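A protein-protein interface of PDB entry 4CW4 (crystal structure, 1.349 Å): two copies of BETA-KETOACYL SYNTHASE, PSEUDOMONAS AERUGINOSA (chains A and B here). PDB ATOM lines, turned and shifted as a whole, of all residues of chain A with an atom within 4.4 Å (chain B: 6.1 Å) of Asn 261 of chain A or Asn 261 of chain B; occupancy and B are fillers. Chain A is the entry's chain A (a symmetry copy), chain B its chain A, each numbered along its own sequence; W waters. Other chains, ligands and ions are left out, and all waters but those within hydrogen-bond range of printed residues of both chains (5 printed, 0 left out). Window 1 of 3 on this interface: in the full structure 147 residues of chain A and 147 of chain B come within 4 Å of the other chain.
The side-chain hydroxyl of Thr 283 of chain B is in hydrogen-bond range of the side-chain amide oxygen of Asn 261 of chain A (2.8 Å).
The backbone carbonyl oxygen of Ser 281 of chain B sits at hydrogen-bond distance from the backbone NH of Thr 283 of chain A (2.9 Å).
The side-chain amide oxygen (OD1) of Asn 261 of chain B is in hydrogen-bond range of the side-chain hydroxyl (OG1) of Thr 283 of chain A.
The backbone carbonyl oxygen of Ser 281 of chain A sits close to the backbone carbonyl oxygen of Ser 281 of chain B, 3.5 Å away.
The backbone carbonyl oxygen of Ser 281 of chain A is in hydrogen-bond range of the backbone NH of Thr 283 of chain B.
OG of Ser 231 of chain A lies within hydrogen-bond range of OG of Ser 231 of chain B (3.2 Å).
The backbone carbonyl oxygen of Ser 226 of chain B sits close to the side-chain hydroxyl of Ser 281 of chain B (3.2 Å).
The backbone carbonyl oxygen (O) of Ser 228 of chain A sits at hydrogen-bond distance from the side-chain amide nitrogen (ND2) of Asn 261 of chain A (3.0 Å).
The backbone NH (N) of Ser 231 of chain B sits at hydrogen-bond distance from the side-chain hydroxyl (OG) of Ser 228 of chain B (3.3 Å).
The backbone NH (N) of Ser 231 of chain A is in hydrogen-bond range of the side-chain hydroxyl (OG) of Ser 228 of chain A.
O of Ser 228 of chain B is in hydrogen-bond range of ND2 of Asn 261 of chain B, at 3.0 Å.
OG of Ser 281 of chain B sits at hydrogen-bond distance from OG1 of Thr 265 of chain B, 2.8 Å away.
Among the printed residues, merely in contact across the chains: Phe 260 of chain A with Ile 229 of chain B (3.5 Å), Phe 260 of chain A with Met 230 of chain B (3.3 Å), Asn 261 of chain A with Asn 261 of chain B (3.7 Å) and Ser 281 of chain A with Ile 282 of chain B (3.4 Å).
Of chain A, only Asn 261 and Thr 283 come within 4 Å of Asn 261 of chain B.
Of the printed residues of chain B, Thr 283 of chain A touches Asn 261 (2.8 Å) and Ser 281 (2.9 Å).
Of the printed residues of chain A, Ile 282 of chain B touches Ser 281.
Thr 265 of chain B touches none of the printed residues of chain A.
Ser 226 of chain B touches none of the printed residues of chain A.
The nearest residue of chain B that does not touch Asn 261 of chain A is Ile 229 of chain B (4.8 Å).
The nearest printed residue of chain A that does not touch Asn 261 of chain B is Ser 228 of chain A (5.3 Å).
The nearest printed residue of chain B that does not touch Phe 260 of chain A is Thr 283 of chain B (6.6 Å).
Printed residues of chain A that touch a printed residue of chain B: Ser 231, Phe 260, Asn 261, Ser 281 and Thr 283.
Hydrophobic or aromatic side chains of chain A within 4 Å of the printed part of chain B: Phe 260.
Of the 18 printed residues of chain B, 7 touch a printed residue of chain A.
Hydrophobic or aromatic side chains of chain B that line the printed part of chain A: Ile 229, Met 230 and Ile 282.
Among the printed residues, 10 pairs touch across the chains.
Among the printed residues, no Asp or Glu carboxylate lies within 4 Å of a Lys or Arg side-chain nitrogen of the other chain.
Asn 261 of chain B touches its own counterpart, Asn 261 of chain A.
Asn 261 of chain A touches Thr 283 of chain B, and with the chains exchanged Thr 283 of chain A touches Asn 261 of chain B.
Ser 281 of chain B touches its own counterpart, Ser 281 of chain A.
Ser 281 of chain A touches Thr 283 of chain B, and with the chains exchanged Thr 283 of chain A touches Ser 281 of chain B.
Positions printed for both chains: 227, 228, 231, 259, 260, 261, 262, 263, 264, 281 and 283.
Water W3 bridges the side-chain hydroxyl (OG) of Ser 281 of chain B (2.7 Å) and the backbone carbonyl oxygen (O) of Thr 283 of chain A (2.8 Å).
Water W2 lies within hydrogen-bond range of the side-chain hydroxyl of Ser 281 of chain A (2.7 Å) and the backbone carbonyl oxygen of Thr 283 of chain B (2.8 Å).
Water W5 lies within hydrogen-bond range of the side-chain hydroxyl of Ser 231 of chain A (2.7 Å), the backbone carbonyl oxygen of Ile 229 of chain B (2.7 Å) and the backbone NH of Asn 261 of chain A (2.9 Å).
Water W4 bridges OD1 of Asn 261 of chain A (2.7 Å) and O of Ile 229 of chain B (2.9 Å).
Water W1 lies within hydrogen-bond range of ND2 of Asn 261 of chain B, ND2 of Asn 261 of chain A, O of Ser 281 of chain A, O of Ser 281 of chain B, OG1 of Thr 283 of chain B and OG1 of Thr 283 of chain A.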
ATOM      1  N   GLY A 227     -28.468  -1.178  14.680  1.00  0.00           N
ATOM      2  CA  GLY A 227     -29.186  -1.672  13.513  1.00  0.00           C
ATOM      3  C   GLY A 227     -30.429  -2.461  13.877  1.00  0.00           C
ATOM      4  O   GLY A 227     -30.837  -2.509  15.039  1.00  0.00           O
ATOM      5  N   SER A 228     -31.050  -3.044  12.857  1.00  0.00           N
ATOM      6  CA  SER A 228     -32.214  -3.932  13.009  1.00  0.00           C
ATOM      7  C   SER A 228     -31.978  -5.142  12.114  1.00  0.00           C
ATOM      8  O   SER A 228     -31.165  -5.070  11.182  1.00  0.00           O
ATOM      9  CB  SER A 228     -33.499  -3.227  12.565  1.00  0.00           C
ATOM     10  OG  SER A 228     -33.428  -2.861  11.185  1.00  0.00           O
ATOM     11  N   SER A 231     -34.853  -4.608   8.739  1.00  0.00           N
ATOM     12  CA  SER A 231     -34.968  -3.261   8.156  1.00  0.00           C
ATOM     13  C   SER A 231     -36.196  -2.613   8.807  1.00  0.00           C
ATOM     14  O   SER A 231     -36.951  -3.283   9.518  1.00  0.00           O
ATOM     15  CB  SER A 231     -35.105  -3.272   6.623  1.00  0.00           C
ATOM     16  OG  SER A 231     -34.067  -4.031   6.011  1.00  0.00           O
ATOM     17  N   GLY A 259     -35.408   3.221   5.461  1.00  0.00           N
ATOM     18  CA  GLY A 259     -35.654   1.816   5.703  1.00  0.00           C
ATOM     19  C   GLY A 259     -34.416   0.979   5.953  1.00  0.00           C
ATOM     20  O   GLY A 259     -34.525  -0.082   6.569  1.00  0.00           O
ATOM     21  N   PHE A 260     -33.250   1.437   5.498  1.00  0.00           N
ATOM     22  CA  PHE A 260     -32.035   0.628   5.601  1.00  0.00           C
ATOM     23  C   PHE A 260     -31.766   0.182   7.033  1.00  0.00           C
ATOM     24  O   PHE A 260     -31.921   0.957   7.989  1.00  0.00           O
ATOM     25  CB  PHE A 260     -30.808   1.394   5.129  1.00  0.00           C
ATOM     26  CG  PHE A 260     -30.745   1.572   3.652  1.00  0.00           C
ATOM     27  CD1 PHE A 260     -30.639   0.474   2.813  1.00  0.00           C
ATOM     28  CD2 PHE A 260     -30.827   2.816   3.086  1.00  0.00           C
ATOM     29  CE1 PHE A 260     -30.595   0.623   1.460  1.00  0.00           C
ATOM     30  CE2 PHE A 260     -30.782   2.954   1.721  1.00  0.00           C
ATOM     31  CZ  PHE A 260     -30.658   1.855   0.915  1.00  0.00           C
ATOM     32  N   ASN A 261     -31.308  -1.057   7.171  1.00  0.00           N
ATOM     33  CA  ASN A 261     -31.084  -1.635   8.503  1.00  0.00           C
ATOM     34  C   ASN A 261     -29.981  -0.957   9.296  1.00  0.00           C
ATOM     35  O   ASN A 261     -29.879  -1.172  10.501  1.00  0.00           O
ATOM     36  CB  ASN A 261     -30.901  -3.160   8.435  1.00  0.00           C
ATOM     37  CG  ASN A 261     -29.463  -3.576   8.280  1.00  0.00           C
ATOM     38  OD1 ASN A 261     -28.707  -3.025   7.481  1.00  0.00           O
ATOM     39  ND2 ASN A 261     -29.082  -4.581   9.055  1.00  0.00           N
ATOM     40  N   SER A 262     -29.171  -0.135   8.628  1.00  0.00           N
ATOM     41  CA  SER A 262     -28.134   0.643   9.317  1.00  0.00           C
ATOM     42  C   SER A 262     -28.625   1.941   9.930  1.00  0.00           C
ATOM     43  O   SER A 262     -27.897   2.589  10.678  1.00  0.00           O
ATOM     44  CB  SER A 262     -26.990   0.964   8.356  1.00  0.00           C
ATOM     45  OG  SER A 262     -27.463   1.763   7.269  1.00  0.00           O
ATOM     46  N   MET A 263     -29.850   2.339   9.610  1.00  0.00           N
ATOM     47  CA  MET A 263     -30.309   3.658  10.012  1.00  0.00           C
ATOM     48  C   MET A 263     -30.420   3.895  11.519  1.00  0.00           C
ATOM     49  O   MET A 263     -30.222   5.027  11.953  1.00  0.00           O
ATOM     50  CB  MET A 263     -31.588   4.036   9.266  1.00  0.00           C
ATOM     51  CG  MET A 263     -31.278   4.362   7.823  1.00  0.00           C
ATOM     52  SD  MET A 263     -30.613   6.056   7.673  1.00  0.00           S
ATOM     53  CE  MET A 263     -29.613   5.924   6.192  1.00  0.00           C
ATOM     54  N   PRO A 264     -30.703   2.850  12.331  1.00  0.00           N
ATOM     55  CA  PRO A 264     -30.639   3.083  13.780  1.00  0.00           C
ATOM     56  C   PRO A 264     -29.250   3.550  14.232  1.00  0.00           C
ATOM     57  O   PRO A 264     -29.144   4.340  15.152  1.00  0.00           O
ATOM     58  CB  PRO A 264     -30.983   1.708  14.368  1.00  0.00           C
ATOM     59  CG  PRO A 264     -31.932   1.132  13.356  1.00  0.00           C
ATOM     60  CD  PRO A 264     -31.316   1.548  12.026  1.00  0.00           C
ATOM     61  N   SER A 281     -23.174  -1.743  11.321  1.00  0.00           N
ATOM     62  CA  SER A 281     -24.374  -2.421  11.779  1.00  0.00           C
ATOM     63  C   SER A 281     -24.225  -3.881  11.438  1.00  0.00           C
ATOM     64  O   SER A 281     -24.240  -4.239  10.266  1.00  0.00           O
ATOM     65  CB  SER A 281     -25.616  -1.852  11.088  1.00  0.00           C
ATOM     66  OG  SER A 281     -25.758  -0.449  11.291  1.00  0.00           O
ATOM     67  N   THR A 283     -25.444  -7.806  11.670  1.00  0.00           N
ATOM     68  CA  THR A 283     -26.559  -8.711  11.930  1.00  0.00           C
ATOM     69  C   THR A 283     -26.151 -10.182  12.017  1.00  0.00           C
ATOM     70  O   THR A 283     -25.195 -10.641  11.384  1.00  0.00           O
ATOM     71  CB  THR A 283     -27.681  -8.541  10.888  1.00  0.00           C
ATOM     72  OG1 THR A 283     -27.147  -8.654   9.568  1.00  0.00           O
ATOM     73  CG2 THR A 283     -28.323  -7.199  11.024  1.00  0.00           C
ATOM     74  N   SER B 226     -20.530 -11.480   4.960  1.00  0.00           N
ATOM     75  CA  SER B 226     -21.187 -11.117   3.700  1.00  0.00           C
ATOM     76  C   SER B 226     -22.484 -10.356   3.989  1.00  0.00           C
ATOM     77  O   SER B 226     -22.591  -9.743   5.038  1.00  0.00           O
ATOM     78  CB  SER B 226     -21.431 -12.343   2.824  1.00  0.00           C
ATOM     79  OG  SER B 226     -21.875 -11.929   1.548  1.00  0.00           O
ATOM     80  N   GLY B 227     -23.434 -10.373   3.057  1.00  0.00           N
ATOM     81  CA  GLY B 227     -24.739  -9.758   3.251  1.00  0.00           C
ATOM     82  C   GLY B 227     -25.151  -8.870   2.093  1.00  0.00           C
ATOM     83  O   GLY B 227     -24.494  -8.837   1.049  1.00  0.00           O
ATOM     84  N   SER B 228     -26.274  -8.183   2.275  1.00  0.00           N
ATOM     85  CA  SER B 228     -26.791  -7.194   1.315  1.00  0.00           C
ATOM     86  C   SER B 228     -27.224  -5.973   2.116  1.00  0.00           C
ATOM     87  O   SER B 228     -27.452  -6.080   3.328  1.00  0.00           O
ATOM     88  CB  SER B 228     -28.002  -7.751   0.560  1.00  0.00           C
ATOM     89  OG  SER B 228     -29.068  -8.057   1.462  1.00  0.00           O
ATOM     90  N   ILE B 229     -27.327  -4.809   1.477  1.00  0.00           N
ATOM     91  CA  ILE B 229     -27.913  -3.665   2.175  1.00  0.00           C
ATOM     92  C   ILE B 229     -29.422  -3.551   2.048  1.00  0.00           C
ATOM     93  O   ILE B 229     -30.048  -2.957   2.914  1.00  0.00           O
ATOM     94  CB  ILE B 229     -27.282  -2.287   1.837  1.00  0.00           C
ATOM     95  CG1 ILE B 229     -27.561  -1.834   0.397  1.00  0.00           C
ATOM     96  CG2 ILE B 229     -25.794  -2.302   2.157  1.00  0.00           C
ATOM     97  CD1 ILE B 229     -27.057  -0.391   0.135  1.00  0.00           C
ATOM     98  N   MET B 230     -30.014  -4.088   0.979  1.00  0.00           N
ATOM     99  CA  MET B 230     -31.466  -3.942   0.788  1.00  0.00           C
ATOM    100  C   MET B 230     -32.315  -4.977   1.518  1.00  0.00           C
ATOM    101  O   MET B 230     -33.513  -4.754   1.692  1.00  0.00           O
ATOM    102  CB  MET B 230     -31.847  -4.000  -0.694  1.00  0.00           C
ATOM    103  CG  MET B 230     -31.157  -2.991  -1.603  1.00  0.00           C
ATOM    104  SD  MET B 230     -31.440  -1.264  -1.170  1.00  0.00           S
ATOM    105  CE  MET B 230     -33.205  -1.223  -1.259  1.00  0.00           C
ATOM    106  N   SER B 231     -31.686  -6.069   1.966  1.00  0.00           N
ATOM    107  CA  SER B 231     -32.342  -7.370   2.178  1.00  0.00           C
ATOM    108  C   SER B 231     -32.660  -7.925   0.785  1.00  0.00           C
ATOM    109  O   SER B 231     -32.510  -7.219  -0.216  1.00  0.00           O
ATOM    110  CB  SER B 231     -33.619  -7.274   3.032  1.00  0.00           C
ATOM    111  OG  SER B 231     -33.378  -6.591   4.259  1.00  0.00           O
ATOM    112  N   GLN B 232     -33.075  -9.184   0.700  1.00  0.00           N
ATOM    113  CA  GLN B 232     -33.479  -9.758  -0.579  1.00  0.00           C
ATOM    114  C   GLN B 232     -34.933  -9.361  -0.805  1.00  0.00           C
ATOM    115  O   GLN B 232     -35.827  -9.855  -0.114  1.00  0.00           O
ATOM    116  CB  GLN B 232     -33.295 -11.280  -0.608  1.00  0.00           C
ATOM    117  CG  GLN B 232     -31.818 -11.743  -0.658  1.00  0.00           C
ATOM    118  CD  GLN B 232     -31.087 -11.490   0.646  1.00  0.00           C
ATOM    119  OE1 GLN B 232     -30.133 -10.713   0.698  1.00  0.00           O
ATOM    120  NE2 GLN B 232     -31.511 -12.165   1.693  1.00  0.00           N
ATOM    121  N   PHE B 238     -38.204 -10.754   0.928  1.00  0.00           N
ATOM    122  CA  PHE B 238     -39.037  -9.731   1.562  1.00  0.00           C
ATOM    123  C   PHE B 238     -40.034  -9.088   0.585  1.00  0.00           C
ATOM    124  O   PHE B 238     -40.988  -8.442   1.023  1.00  0.00           O
ATOM    125  CB  PHE B 238     -38.214  -8.623   2.226  1.00  0.00           C
ATOM    126  CG  PHE B 238     -37.659  -8.961   3.597  1.00  0.00           C
ATOM    127  CD1 PHE B 238     -37.743 -10.237   4.137  1.00  0.00           C
ATOM    128  CD2 PHE B 238     -37.047  -7.972   4.346  1.00  0.00           C
ATOM    129  CE1 PHE B 238     -37.219 -10.530   5.398  1.00  0.00           C
ATOM    130  CE2 PHE B 238     -36.522  -8.261   5.610  1.00  0.00           C
ATOM    131  CZ  PHE B 238     -36.611  -9.540   6.133  1.00  0.00           C
ATOM    132  N   GLY B 259     -35.340 -13.646   3.222  1.00  0.00           N
ATOM    133  CA  GLY B 259     -35.168 -12.236   2.944  1.00  0.00           C
ATOM    134  C   GLY B 259     -34.125 -11.536   3.790  1.00  0.00           C
ATOM    135  O   GLY B 259     -33.611 -10.499   3.369  1.00  0.00           O
ATOM    136  N   PHE B 260     -33.800 -12.082   4.961  1.00  0.00           N
ATOM    137  CA  PHE B 260     -32.888 -11.401   5.880  1.00  0.00           C
ATOM    138  C   PHE B 260     -31.563 -11.051   5.214  1.00  0.00           C
ATOM    139  O   PHE B 260     -30.990 -11.850   4.458  1.00  0.00           O
ATOM    140  CB  PHE B 260     -32.568 -12.260   7.095  1.00  0.00           C
ATOM    141  CG  PHE B 260     -33.696 -12.374   8.061  1.00  0.00           C
ATOM    142  CD1 PHE B 260     -34.177 -11.254   8.719  1.00  0.00           C
ATOM    143  CD2 PHE B 260     -34.308 -13.576   8.294  1.00  0.00           C
ATOM    144  CE1 PHE B 260     -35.217 -11.343   9.594  1.00  0.00           C
ATOM    145  CE2 PHE B 260     -35.356 -13.654   9.177  1.00  0.00           C
ATOM    146  CZ  PHE B 260     -35.800 -12.536   9.828  1.00  0.00           C
ATOM    147  N   ASN B 261     -31.052  -9.869   5.542  1.00  0.00           N
ATOM    148  CA  ASN B 261     -29.820  -9.378   4.908  1.00  0.00           C
ATOM    149  C   ASN B 261     -28.584 -10.196   5.239  1.00  0.00           C
ATOM    150  O   ASN B 261     -27.562 -10.048   4.575  1.00  0.00           O
ATOM    151  CB  ASN B 261     -29.612  -7.877   5.165  1.00  0.00           C
ATOM    152  CG  ASN B 261     -28.800  -7.595   6.400  1.00  0.00           C
ATOM    153  OD1 ASN B 261     -29.006  -8.179   7.464  1.00  0.00           O
ATOM    154  ND2 ASN B 261     -27.864  -6.669   6.259  1.00  0.00           N
ATOM    155  N   SER B 262     -28.681 -11.061   6.250  1.00  0.00           N
ATOM    156  CA  SER B 262     -27.577 -11.966   6.589  1.00  0.00           C
ATOM    157  C   SER B 262     -27.530 -13.237   5.763  1.00  0.00           C
ATOM    158  O   SER B 262     -26.559 -13.987   5.831  1.00  0.00           O
ATOM    159  CB  SER B 262     -27.647 -12.352   8.067  1.00  0.00           C
ATOM    160  OG  SER B 262     -28.864 -13.050   8.342  1.00  0.00           O
ATOM    161  N   MET B 263     -28.577 -13.500   4.991  1.00  0.00           N
ATOM    162  CA  MET B 263     -28.677 -14.786   4.322  1.00  0.00           C
ATOM    163  C   MET B 263     -27.595 -15.080   3.280  1.00  0.00           C
ATOM    164  O   MET B 263     -27.244 -16.246   3.110  1.00  0.00           O
ATOM    165  CB  MET B 263     -30.087 -15.003   3.775  1.00  0.00           C
ATOM    166  CG  MET B 263     -31.050 -15.290   4.904  1.00  0.00           C
ATOM    167  SD  MET B 263     -30.918 -17.032   5.437  1.00  0.00           S
ATOM    168  CE  MET B 263     -31.438 -16.928   7.149  1.00  0.00           C
ATOM    169  N   PRO B 264     -27.039 -14.052   2.600  1.00  0.00           N
ATOM    170  CA  PRO B 264     -25.893 -14.357   1.732  1.00  0.00           C
ATOM    171  C   PRO B 264     -24.724 -14.977   2.509  1.00  0.00           C
ATOM    172  O   PRO B 264     -24.020 -15.816   1.978  1.00  0.00           O
ATOM    173  CB  PRO B 264     -25.515 -12.985   1.160  1.00  0.00           C
ATOM    174  CG  PRO B 264     -26.836 -12.273   1.082  1.00  0.00           C
ATOM    175  CD  PRO B 264     -27.529 -12.684   2.375  1.00  0.00           C
ATOM    176  N   THR B 265     -24.553 -14.566   3.758  1.00  0.00           N
ATOM    177  CA  THR B 265     -23.554 -15.107   4.675  1.00  0.00           C
ATOM    178  C   THR B 265     -23.993 -16.474   5.216  1.00  0.00           C
ATOM    179  O   THR B 265     -23.239 -17.448   5.190  1.00  0.00           O
ATOM    180  CB  THR B 265     -23.409 -14.144   5.880  1.00  0.00           C
ATOM    181  OG1 THR B 265     -23.223 -12.819   5.373  1.00  0.00           O
ATOM    182  CG2 THR B 265     -22.252 -14.568   6.778  1.00  0.00           C
ATOM    183  N   SER B 281     -22.710 -10.168   9.307  1.00  0.00           N
ATOM    184  CA  SER B 281     -23.032  -9.398   8.118  1.00  0.00           C
ATOM    185  C   SER B 281     -23.063  -7.945   8.514  1.00  0.00           C
ATOM    186  O   SER B 281     -23.950  -7.533   9.254  1.00  0.00           O
ATOM    187  CB  SER B 281     -24.395  -9.812   7.556  1.00  0.00           C
ATOM    188  OG  SER B 281     -24.461 -11.202   7.254  1.00  0.00           O
ATOM    189  N   ILE B 282     -22.097  -7.179   8.007  1.00  0.00           N
ATOM    190  CA  ILE B 282     -21.919  -5.794   8.414  1.00  0.00           C
ATOM    191  C   ILE B 282     -22.359  -4.871   7.306  1.00  0.00           C
ATOM    192  O   ILE B 282     -21.944  -5.039   6.179  1.00  0.00           O
ATOM    193  CB  ILE B 282     -20.471  -5.508   8.804  1.00  0.00           C
ATOM    194  CG1 ILE B 282     -19.974  -6.623   9.723  1.00  0.00           C
ATOM    195  CG2 ILE B 282     -20.361  -4.145   9.475  1.00  0.00           C
ATOM    196  CD1 ILE B 282     -18.591  -6.430  10.256  1.00  0.00           C
ATOM    197  N   THR B 283     -23.259  -3.936   7.603  1.00  0.00           N
ATOM    198  CA  THR B 283     -23.661  -2.940   6.614  1.00  0.00           C
ATOM    199  C   THR B 283     -23.198  -1.522   6.946  1.00  0.00           C
ATOM    200  O   THR B 283     -23.053  -1.128   8.108  1.00  0.00           O
ATOM    201  CB  THR B 283     -25.184  -2.952   6.385  1.00  0.00           C
ATOM    202  OG1 THR B 283     -25.870  -2.831   7.633  1.00  0.00           O
ATOM    203  CG2 THR B 283     -25.606  -4.231   5.738  1.00  0.00           C
HETATM  204  O   HOH W   1     -26.340  -5.752   8.681  1.00  0.00           O
HETATM  205  O   HOH W   2     -23.928   0.886   9.865  1.00  0.00           O
HETATM  206  O   HOH W   3     -24.565 -12.640   9.509  1.00  0.00           O
HETATM  207  O   HOH W   4     -28.716  -1.674   5.090  1.00  0.00           O
HETATM  208  O   HOH W   5     -31.779  -2.917   5.031  1.00  0.00           O
